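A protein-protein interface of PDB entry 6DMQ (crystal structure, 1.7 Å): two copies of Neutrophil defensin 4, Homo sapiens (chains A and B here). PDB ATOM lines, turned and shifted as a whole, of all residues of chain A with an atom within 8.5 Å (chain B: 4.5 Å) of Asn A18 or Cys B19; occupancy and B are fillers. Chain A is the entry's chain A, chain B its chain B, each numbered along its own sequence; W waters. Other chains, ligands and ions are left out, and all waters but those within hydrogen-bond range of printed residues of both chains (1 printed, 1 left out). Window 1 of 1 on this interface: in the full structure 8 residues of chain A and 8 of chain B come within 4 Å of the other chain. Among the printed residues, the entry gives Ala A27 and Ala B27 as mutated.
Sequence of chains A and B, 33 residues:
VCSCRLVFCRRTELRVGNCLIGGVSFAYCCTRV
Water W1 bridges O of Cys A2 (2.5 Å) and OH of Tyr B28 (3.0 Å).
Among the printed residues, merely in contact across the chains: Cys A19 with Asn B18 (3.1 Å), Asn A18 with Cys B19 (3.2 Å), Gly A17 with Leu B20 (3.3 Å), Val A16 with Ile B21 (3.6 Å), Ile A21 with Tyr B28 (3.7 Å) and Tyr A28 with Ile B21 (3.8 Å).
Cys B19 touches one residue of chain A. Printed residues of chain A within 4 Å of Cys B4: Tyr A28 (3.3 Å). Printed residues of chain A within 4 Å of Tyr B28: Cys A4 (3.3 Å) and Ile A21 (3.7 Å). Of the printed residues of chain B, Gly A17 touches Leu B20 (3.3 Å). The nearest residue of chain B that does not touch Asn A18 is Asn B18 (4.2 Å). The nearest residue of chain A that does not touch Cys B19 is Cys A19 (4.3 Å). The nearest printed residue of chain B that does not touch Leu A20 is Cys B19 (5.0 Å).
Printed residues of chain B that touch a printed residue of chain A: Cys B4, Asn B18, Cys B19, Leu B20, Ile B21 and Tyr B28. Along chain B the printed residues that touch a printed residue of chain A span positions 4 to 28. Among the printed residues, no Asp or Glu carboxylate lies within 4 Å of a Lys or Arg side-chain nitrogen of the other chain.
Cys A4 touches Tyr B28, and with the chains exchanged Tyr A28 touches Cys B4. Asn A18 touches Cys B19, and with the chains exchanged Cys A19 touches Asn B18. Asn A18 touches Leu B20, and with the chains exchanged Leu A20 touches Asn B18. Ile A21 touches Tyr B28, and with the chains exchanged Tyr A28 touches Ile B21. 10 positions are printed for both chains. Of the 10 pairs that touch across the chains among the printed residues, 8 have their exchanged pair printed and touching as well.
The side-chain sulfur (SG) of Cys A4 sits close to the side-chain hydroxyl (OH) of Tyr B28, 3.3 Å away. The backbone NH (N) of Leu B20 sits at hydrogen-bond distance from the backbone carbonyl oxygen (O) of Asn A18 (2.6 Å). The backbone NH of Leu A20 lies within hydrogen-bond range of the backbone carbonyl oxygen of Asn B18 (2.8 Å). OH of Tyr A28 lies close to SG of Cys B4 (3.3 Å).
OH of Tyr A28 sits close to SG of Cys A2 (3.8 Å). SG of Cys A4 forms a disulfide with SG of Cys A19. N of Val A16 is in hydrogen-bond range of O of Tyr A28 (2.7 Å). OD1 of Asn A18 lies close to O of Phe A26 (3.3 Å). The side-chain sulfur (SG) of Cys B4 forms a disulfide with the side-chain sulfur (SG) of Cys B19, 2.0 Å away. The backbone NH of Cys B19 lies within hydrogen-bond range of the backbone carbonyl oxygen of Phe B26 (2.8 Å).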
ATOM      1  N   CYS A   2     -27.995 -10.128 -14.122  1.00  0.00           N
ATOM      2  CA  CYS A   2     -26.958 -10.039 -15.136  1.00  0.00           C
ATOM      3  C   CYS A   2     -25.597 -10.442 -14.573  1.00  0.00           C
ATOM      4  O   CYS A   2     -25.214 -10.050 -13.472  1.00  0.00           O
ATOM      5  CB  CYS A   2     -26.809  -8.608 -15.650  1.00  0.00           C
ATOM      6  SG  CYS A   2     -28.330  -7.906 -16.295  1.00  0.00           S
ATOM      7  N   SER A   3     -24.820 -11.133 -15.408  1.00  0.00           N
ATOM      8  CA  SER A   3     -23.449 -11.520 -15.101  1.00  0.00           C
ATOM      9  C   SER A   3     -22.528 -11.395 -16.334  1.00  0.00           C
ATOM     10  O   SER A   3     -22.908 -11.688 -17.468  1.00  0.00           O
ATOM     11  CB  SER A   3     -23.430 -12.918 -14.570  1.00  0.00           C
ATOM     12  OG  SER A   3     -24.716 -13.272 -14.113  1.00  0.00           O
ATOM     13  N   CYS A   4     -21.270 -11.032 -16.094  1.00  0.00           N
ATOM     14  CA  CYS A   4     -20.246 -11.172 -17.080  1.00  0.00           C
ATOM     15  C   CYS A   4     -19.778 -12.623 -17.119  1.00  0.00           C
ATOM     16  O   CYS A   4     -19.304 -13.081 -16.108  1.00  0.00           O
ATOM     17  CB  CYS A   4     -19.047 -10.263 -16.858  1.00  0.00           C
ATOM     18  SG  CYS A   4     -19.510  -8.530 -16.625  1.00  0.00           S
ATOM     19  N   ARG A   5     -19.869 -13.232 -18.318  1.00  0.00           N
ATOM     20  CA  ARG A   5     -19.467 -14.595 -18.615  1.00  0.00           C
ATOM     21  C   ARG A   5     -18.383 -14.590 -19.698  1.00  0.00           C
ATOM     22  O   ARG A   5     -18.401 -13.738 -20.588  1.00  0.00           O
ATOM     23  CB  ARG A   5     -20.701 -15.389 -19.025  1.00  0.00           C
ATOM     24  CG  ARG A   5     -21.825 -15.288 -18.010  1.00  0.00           C
ATOM     25  CD  ARG A   5     -22.839 -16.377 -18.240  1.00  0.00           C
ATOM     26  NE  ARG A   5     -23.972 -16.412 -17.313  1.00  0.00           N
ATOM     27  CZ  ARG A   5     -23.901 -16.684 -16.004  1.00  0.00           C
ATOM     28  NH1 ARG A   5     -22.734 -16.929 -15.430  1.00  0.00           N
ATOM     29  NH2 ARG A   5     -24.994 -16.682 -15.259  1.00  0.00           N
ATOM     30  N   LEU A   6     -17.406 -15.499 -19.535  1.00  0.00           N
ATOM     31  CA  LEU A   6     -16.216 -15.529 -20.372  1.00  0.00           C
ATOM     32  C   LEU A   6     -16.565 -15.777 -21.848  1.00  0.00           C
ATOM     33  O   LEU A   6     -15.938 -15.204 -22.748  1.00  0.00           O
ATOM     34  CB  LEU A   6     -15.227 -16.568 -19.819  1.00  0.00           C
ATOM     35  CG  LEU A   6     -14.600 -16.207 -18.463  1.00  0.00           C
ATOM     36  CD1 LEU A   6     -13.961 -17.387 -17.715  1.00  0.00           C
ATOM     37  CD2 LEU A   6     -13.579 -15.131 -18.677  1.00  0.00           C
ATOM     38  N   VAL A   7     -17.539 -16.639 -22.124  1.00  0.00           N
ATOM     39  CA  VAL A   7     -17.779 -17.124 -23.479  1.00  0.00           C
ATOM     40  C   VAL A   7     -19.247 -16.835 -23.881  1.00  0.00           C
ATOM     41  O   VAL A   7     -19.562 -15.762 -24.506  1.00  0.00           O
ATOM     42  CB  VAL A   7     -17.354 -18.599 -23.585  1.00  0.00           C
ATOM     43  CG1 VAL A   7     -17.525 -19.149 -24.988  1.00  0.00           C
ATOM     44  CG2 VAL A   7     -15.935 -18.803 -23.113  1.00  0.00           C
ATOM     45  N   ARG A  15     -27.674 -11.654 -24.431  1.00  0.00           N
ATOM     46  CA  ARG A  15     -26.405 -10.945 -24.453  1.00  0.00           C
ATOM     47  C   ARG A  15     -26.638  -9.446 -24.680  1.00  0.00           C
ATOM     48  O   ARG A  15     -26.682  -8.989 -25.822  1.00  0.00           O
ATOM     49  CB  ARG A  15     -25.481 -11.498 -25.534  1.00  0.00           C
ATOM     50  CG  ARG A  15     -24.065 -10.971 -25.361  1.00  0.00           C
ATOM     51  CD  ARG A  15     -23.322 -10.980 -26.681  1.00  0.00           C
ATOM     52  NE  ARG A  15     -23.736  -9.861 -27.518  1.00  0.00           N
ATOM     53  CZ  ARG A  15     -23.287  -8.619 -27.402  1.00  0.00           C
ATOM     54  NH1 ARG A  15     -22.582  -8.266 -26.348  1.00  0.00           N
ATOM     55  NH2 ARG A  15     -23.532  -7.726 -28.345  1.00  0.00           N
ATOM     56  N   VAL A  16     -26.659  -8.701 -23.573  1.00  0.00           N
ATOM     57  CA  VAL A  16     -27.103  -7.250 -23.494  1.00  0.00           C
ATOM     58  C   VAL A  16     -25.911  -6.350 -23.866  1.00  0.00           C
ATOM     59  O   VAL A  16     -26.059  -5.253 -24.347  1.00  0.00           O
ATOM     60  CB  VAL A  16     -27.613  -6.910 -22.064  1.00  0.00           C
ATOM     61  CG1 VAL A  16     -27.862  -5.427 -21.868  1.00  0.00           C
ATOM     62  CG2 VAL A  16     -28.894  -7.674 -21.730  1.00  0.00           C
ATOM     63  N   GLY A  17     -24.700  -6.825 -23.629  1.00  0.00           N
ATOM     64  CA  GLY A  17     -23.502  -6.012 -23.992  1.00  0.00           C
ATOM     65  C   GLY A  17     -22.253  -6.758 -23.703  1.00  0.00           C
ATOM     66  O   GLY A  17     -22.287  -7.992 -23.749  1.00  0.00           O
ATOM     67  N   ASN A  18     -21.187  -6.060 -23.315  1.00  0.00           N
ATOM     68  CA  ASN A  18     -19.849  -6.621 -23.072  1.00  0.00           C
ATOM     69  C   ASN A  18     -19.283  -6.112 -21.732  1.00  0.00           C
ATOM     70  O   ASN A  18     -19.736  -5.012 -21.203  1.00  0.00           O
ATOM     71  CB  ASN A  18     -18.873  -6.288 -24.213  1.00  0.00           C
ATOM     72  CG  ASN A  18     -19.284  -7.026 -25.467  1.00  0.00           C
ATOM     73  OD1 ASN A  18     -19.019  -8.215 -25.581  1.00  0.00           O
ATOM     74  ND2 ASN A  18     -20.134  -6.396 -26.252  1.00  0.00           N
ATOM     75  N   CYS A  19     -18.352  -6.869 -21.153  1.00  0.00           N
ATOM     76  CA  CYS A  19     -17.550  -6.336 -20.017  1.00  0.00           C
ATOM     77  C   CYS A  19     -16.069  -6.428 -20.412  1.00  0.00           C
ATOM     78  O   CYS A  19     -15.678  -7.258 -21.202  1.00  0.00           O
ATOM     79  CB  CYS A  19     -17.776  -7.144 -18.729  1.00  0.00           C
ATOM     80  SG  CYS A  19     -19.428  -7.875 -18.535  1.00  0.00           S
ATOM     81  N   LEU A  20     -15.312  -5.602 -19.731  1.00  0.00           N
ATOM     82  CA  LEU A  20     -13.862  -5.563 -19.845  1.00  0.00           C
ATOM     83  C   LEU A  20     -13.365  -5.542 -18.404  1.00  0.00           C
ATOM     84  O   LEU A  20     -13.588  -4.624 -17.736  1.00  0.00           O
ATOM     85  CB  LEU A  20     -13.424  -4.326 -20.630  1.00  0.00           C
ATOM     86  CG  LEU A  20     -11.916  -4.192 -20.811  1.00  0.00           C
ATOM     87  CD1 LEU A  20     -11.343  -5.373 -21.593  1.00  0.00           C
ATOM     88  CD2 LEU A  20     -11.604  -2.896 -21.531  1.00  0.00           C
ATOM     89  N   ILE A  21     -12.821  -6.664 -17.994  1.00  0.00           N
ATOM     90  CA  ILE A  21     -12.292  -6.859 -16.692  1.00  0.00           C
ATOM     91  C   ILE A  21     -10.855  -7.419 -16.803  1.00  0.00           C
ATOM     92  O   ILE A  21     -10.628  -8.474 -17.384  1.00  0.00           O
ATOM     93  CB  ILE A  21     -13.163  -7.863 -15.893  1.00  0.00           C
ATOM     94  CG1 ILE A  21     -14.649  -7.470 -15.913  1.00  0.00           C
ATOM     95  CG2 ILE A  21     -12.549  -8.034 -14.498  1.00  0.00           C
ATOM     96  CD1 ILE A  21     -15.619  -8.494 -15.265  1.00  0.00           C
ATOM     97  N   VAL A  24      -9.543  -8.706 -20.047  1.00  0.00           N
ATOM     98  CA  VAL A  24     -10.331  -9.757 -20.721  1.00  0.00           C
ATOM     99  C   VAL A  24     -11.758  -9.241 -21.019  1.00  0.00           C
ATOM    100  O   VAL A  24     -12.429  -8.732 -20.167  1.00  0.00           O
ATOM    101  CB  VAL A  24     -10.324 -11.062 -19.875  1.00  0.00           C
ATOM    102  CG1 VAL A  24     -10.960 -12.222 -20.582  1.00  0.00           C
ATOM    103  CG2 VAL A  24      -8.910 -11.458 -19.501  1.00  0.00           C
ATOM    104  N   SER A  25     -12.262  -9.567 -22.220  1.00  0.00           N
ATOM    105  CA  SER A  25     -13.614  -9.210 -22.624  1.00  0.00           C
ATOM    106  C   SER A  25     -14.548 -10.392 -22.358  1.00  0.00           C
ATOM    107  O   SER A  25     -14.132 -11.523 -22.563  1.00  0.00           O
ATOM    108  CB  SER A  25     -13.617  -8.873 -24.085  1.00  0.00           C
ATOM    109  OG  SER A  25     -12.852  -7.696 -24.332  1.00  0.00           O
ATOM    110  N   PHE A  26     -15.770 -10.097 -21.905  1.00  0.00           N
ATOM    111  CA  PHE A  26     -16.823 -10.979 -21.450  1.00  0.00           C
ATOM    112  C   PHE A  26     -18.121 -10.588 -22.165  1.00  0.00           C
ATOM    113  O   PHE A  26     -18.293  -9.415 -22.631  1.00  0.00           O
ATOM    114  CB  PHE A  26     -17.116 -10.818 -19.966  1.00  0.00           C
ATOM    115  CG  PHE A  26     -15.999 -11.154 -19.012  1.00  0.00           C
ATOM    116  CD1 PHE A  26     -14.866 -10.356 -18.949  1.00  0.00           C
ATOM    117  CD2 PHE A  26     -16.100 -12.238 -18.145  1.00  0.00           C
ATOM    118  CE1 PHE A  26     -13.814 -10.693 -18.113  1.00  0.00           C
ATOM    119  CE2 PHE A  26     -15.085 -12.513 -17.237  1.00  0.00           C
ATOM    120  CZ  PHE A  26     -13.923 -11.779 -17.267  1.00  0.00           C
ATOM    121  N   ALA A  27     -18.963 -11.591 -22.379  1.00  0.00           N
ATOM    122  CA  ALA A  27     -20.355 -11.369 -22.708  1.00  0.00           C
ATOM    123  C   ALA A  27     -21.007 -10.840 -21.455  1.00  0.00           C
ATOM    124  O   ALA A  27     -20.655 -11.353 -20.320  1.00  0.00           O
ATOM    125  CB  ALA A  27     -21.044 -12.647 -23.126  1.00  0.00           C
ATOM    126  N   TYR A  28     -21.804  -9.774 -21.622  1.00  0.00           N
ATOM    127  CA  TYR A  28     -22.695  -9.296 -20.529  1.00  0.00           C
ATOM    128  C   TYR A  28     -24.090  -9.897 -20.781  1.00  0.00           C
ATOM    129  O   TYR A  28     -24.787  -9.511 -21.750  1.00  0.00           O
ATOM    130  CB  TYR A  28     -22.776  -7.752 -20.436  1.00  0.00           C
ATOM    131  CG  TYR A  28     -23.465  -7.246 -19.194  1.00  0.00           C
ATOM    132  CD1 TYR A  28     -23.042  -7.636 -17.912  1.00  0.00           C
ATOM    133  CD2 TYR A  28     -24.497  -6.327 -19.251  1.00  0.00           C
ATOM    134  CE1 TYR A  28     -23.650  -7.168 -16.745  1.00  0.00           C
ATOM    135  CE2 TYR A  28     -25.158  -5.892 -18.111  1.00  0.00           C
ATOM    136  CZ  TYR A  28     -24.686  -6.262 -16.861  1.00  0.00           C
ATOM    137  OH  TYR A  28     -25.263  -5.745 -15.777  1.00  0.00           O
ATOM    138  N   CYS A  29     -24.542 -10.761 -19.852  1.00  0.00           N
ATOM    139  CA  CYS A  29     -25.662 -11.669 -20.039  1.00  0.00           C
ATOM    140  C   CYS A  29     -26.743 -11.413 -18.980  1.00  0.00           C
ATOM    141  O   CYS A  29     -26.438 -11.442 -17.790  1.00  0.00           O
ATOM    142  CB  CYS A  29     -25.208 -13.127 -19.897  1.00  0.00           C
ATOM    143  SG  CYS A  29     -23.771 -13.567 -20.919  1.00  0.00           S
ATOM    144  N   CYS B   4     -23.748  -2.803 -13.094  1.00  0.00           N
ATOM    145  CA  CYS B   4     -23.220  -1.885 -14.125  1.00  0.00           C
ATOM    146  C   CYS B   4     -23.866  -0.532 -13.836  1.00  0.00           C
ATOM    147  O   CYS B   4     -25.083  -0.479 -13.762  1.00  0.00           O
ATOM    148  CB  CYS B   4     -23.497  -2.386 -15.556  1.00  0.00           C
ATOM    149  SG  CYS B   4     -22.542  -3.830 -16.139  1.00  0.00           S
ATOM    150  N   ASN B  18     -15.352  -2.513 -16.641  1.00  0.00           N
ATOM    151  CA  ASN B  18     -16.267  -1.716 -17.383  1.00  0.00           C
ATOM    152  C   ASN B  18     -17.286  -2.619 -18.062  1.00  0.00           C
ATOM    153  O   ASN B  18     -16.961  -3.787 -18.332  1.00  0.00           O
ATOM    154  CB  ASN B  18     -15.566  -0.851 -18.424  1.00  0.00           C
ATOM    155  CG  ASN B  18     -15.001   0.401 -17.785  1.00  0.00           C
ATOM    156  OD1 ASN B  18     -14.165   0.330 -16.901  1.00  0.00           O
ATOM    157  ND2 ASN B  18     -15.435   1.566 -18.216  1.00  0.00           N
ATOM    158  N   CYS B  19     -18.482  -2.053 -18.256  1.00  0.00           N
ATOM    159  CA  CYS B  19     -19.482  -2.660 -19.073  1.00  0.00           C
ATOM    160  C   CYS B  19     -19.511  -1.841 -20.338  1.00  0.00           C
ATOM    161  O   CYS B  19     -19.299  -0.675 -20.233  1.00  0.00           O
ATOM    162  CB  CYS B  19     -20.830  -2.730 -18.366  1.00  0.00           C
ATOM    163  SG  CYS B  19     -20.680  -3.324 -16.658  1.00  0.00           S
ATOM    164  N   LEU B  20     -19.918  -2.453 -21.405  1.00  0.00           N
ATOM    165  CA  LEU B  20     -20.238  -1.661 -22.588  1.00  0.00           C
ATOM    166  C   LEU B  20     -21.612  -2.173 -23.046  1.00  0.00           C
ATOM    167  O   LEU B  20     -21.760  -3.317 -23.350  1.00  0.00           O
ATOM    168  CB  LEU B  20     -19.184  -1.788 -23.691  1.00  0.00           C
ATOM    169  CG  LEU B  20     -19.502  -0.877 -24.874  1.00  0.00           C
ATOM    170  CD1 LEU B  20     -19.108   0.556 -24.618  1.00  0.00           C
ATOM    171  CD2 LEU B  20     -18.922  -1.417 -26.152  1.00  0.00           C
ATOM    172  N   ILE B  21     -22.561  -1.284 -23.020  1.00  0.00           N
ATOM    173  CA  ILE B  21     -23.980  -1.522 -23.328  1.00  0.00           C
ATOM    174  C   ILE B  21     -24.549  -0.399 -24.208  1.00  0.00           C
ATOM    175  O   ILE B  21     -24.693   0.713 -23.752  1.00  0.00           O
ATOM    176  CB  ILE B  21     -24.843  -1.685 -22.063  1.00  0.00           C
ATOM    177  CG1 ILE B  21     -24.281  -2.632 -21.005  1.00  0.00           C
ATOM    178  CG2 ILE B  21     -26.227  -2.153 -22.470  1.00  0.00           C
ATOM    179  CD1 ILE B  21     -24.887  -2.416 -19.626  1.00  0.00           C
ATOM    180  N   VAL B  24     -22.285   2.614 -24.764  1.00  0.00           N
ATOM    181  CA  VAL B  24     -22.067   3.401 -23.570  1.00  0.00           C
ATOM    182  C   VAL B  24     -21.218   2.577 -22.585  1.00  0.00           C
ATOM    183  O   VAL B  24     -21.426   1.366 -22.362  1.00  0.00           O
ATOM    184  CB  VAL B  24     -23.408   3.876 -22.946  1.00  0.00           C
ATOM    185  CG1 VAL B  24     -23.179   4.532 -21.567  1.00  0.00           C
ATOM    186  CG2 VAL B  24     -24.202   4.823 -23.843  1.00  0.00           C
ATOM    187  N   SER B  25     -20.281   3.273 -21.935  1.00  0.00           N
ATOM    188  CA  SER B  25     -19.446   2.704 -20.928  1.00  0.00           C
ATOM    189  C   SER B  25     -20.118   2.872 -19.564  1.00  0.00           C
ATOM    190  O   SER B  25     -20.723   3.925 -19.228  1.00  0.00           O
ATOM    191  CB  SER B  25     -18.090   3.367 -20.967  1.00  0.00           C
ATOM    192  OG  SER B  25     -17.049   2.541 -20.444  1.00  0.00           O
ATOM    193  N   PHE B  26     -19.994   1.837 -18.748  1.00  0.00           N
ATOM    194  CA  PHE B  26     -20.453   1.866 -17.329  1.00  0.00           C
ATOM    195  C   PHE B  26     -19.338   1.278 -16.472  1.00  0.00           C
ATOM    196  O   PHE B  26     -18.519   0.492 -17.006  1.00  0.00           O
ATOM    197  CB  PHE B  26     -21.692   0.985 -17.125  1.00  0.00           C
ATOM    198  CG  PHE B  26     -22.874   1.457 -17.917  1.00  0.00           C
ATOM    199  CD1 PHE B  26     -23.019   0.965 -19.200  1.00  0.00           C
ATOM    200  CD2 PHE B  26     -23.837   2.328 -17.433  1.00  0.00           C
ATOM    201  CE1 PHE B  26     -24.001   1.476 -20.011  1.00  0.00           C
ATOM    202  CE2 PHE B  26     -24.858   2.798 -18.269  1.00  0.00           C
ATOM    203  CZ  PHE B  26     -24.997   2.254 -19.519  1.00  0.00           C
ATOM    204  N   ALA B  27     -19.209   1.759 -15.233  1.00  0.00           N
ATOM    205  CA  ALA B  27     -18.315   1.108 -14.297  1.00  0.00           C
ATOM    206  C   ALA B  27     -18.930  -0.239 -13.900  1.00  0.00           C
ATOM    207  O   ALA B  27     -20.164  -0.366 -13.710  1.00  0.00           O
ATOM    208  CB  ALA B  27     -18.140   1.945 -13.076  1.00  0.00           C
ATOM    209  N   TYR B  28     -18.076  -1.240 -13.735  1.00  0.00           N
ATOM    210  CA  TYR B  28     -18.533  -2.555 -13.252  1.00  0.00           C
ATOM    211  C   TYR B  28     -18.085  -2.598 -11.789  1.00  0.00           C
ATOM    212  O   TYR B  28     -16.861  -2.629 -11.608  1.00  0.00           O
ATOM    213  CB  TYR B  28     -17.920  -3.723 -14.019  1.00  0.00           C
ATOM    214  CG  TYR B  28     -18.657  -5.022 -13.854  1.00  0.00           C
ATOM    215  CD1 TYR B  28     -20.032  -5.110 -14.029  1.00  0.00           C
ATOM    216  CD2 TYR B  28     -17.962  -6.156 -13.478  1.00  0.00           C
ATOM    217  CE1 TYR B  28     -20.717  -6.313 -13.900  1.00  0.00           C
ATOM    218  CE2 TYR B  28     -18.628  -7.366 -13.361  1.00  0.00           C
ATOM    219  CZ  TYR B  28     -20.006  -7.430 -13.555  1.00  0.00           C
ATOM    220  OH  TYR B  28     -20.569  -8.668 -13.450  1.00  0.00           O
HETATM  221  O   HOH W   1     -23.561  -8.273 -13.030  1.00  0.00           O
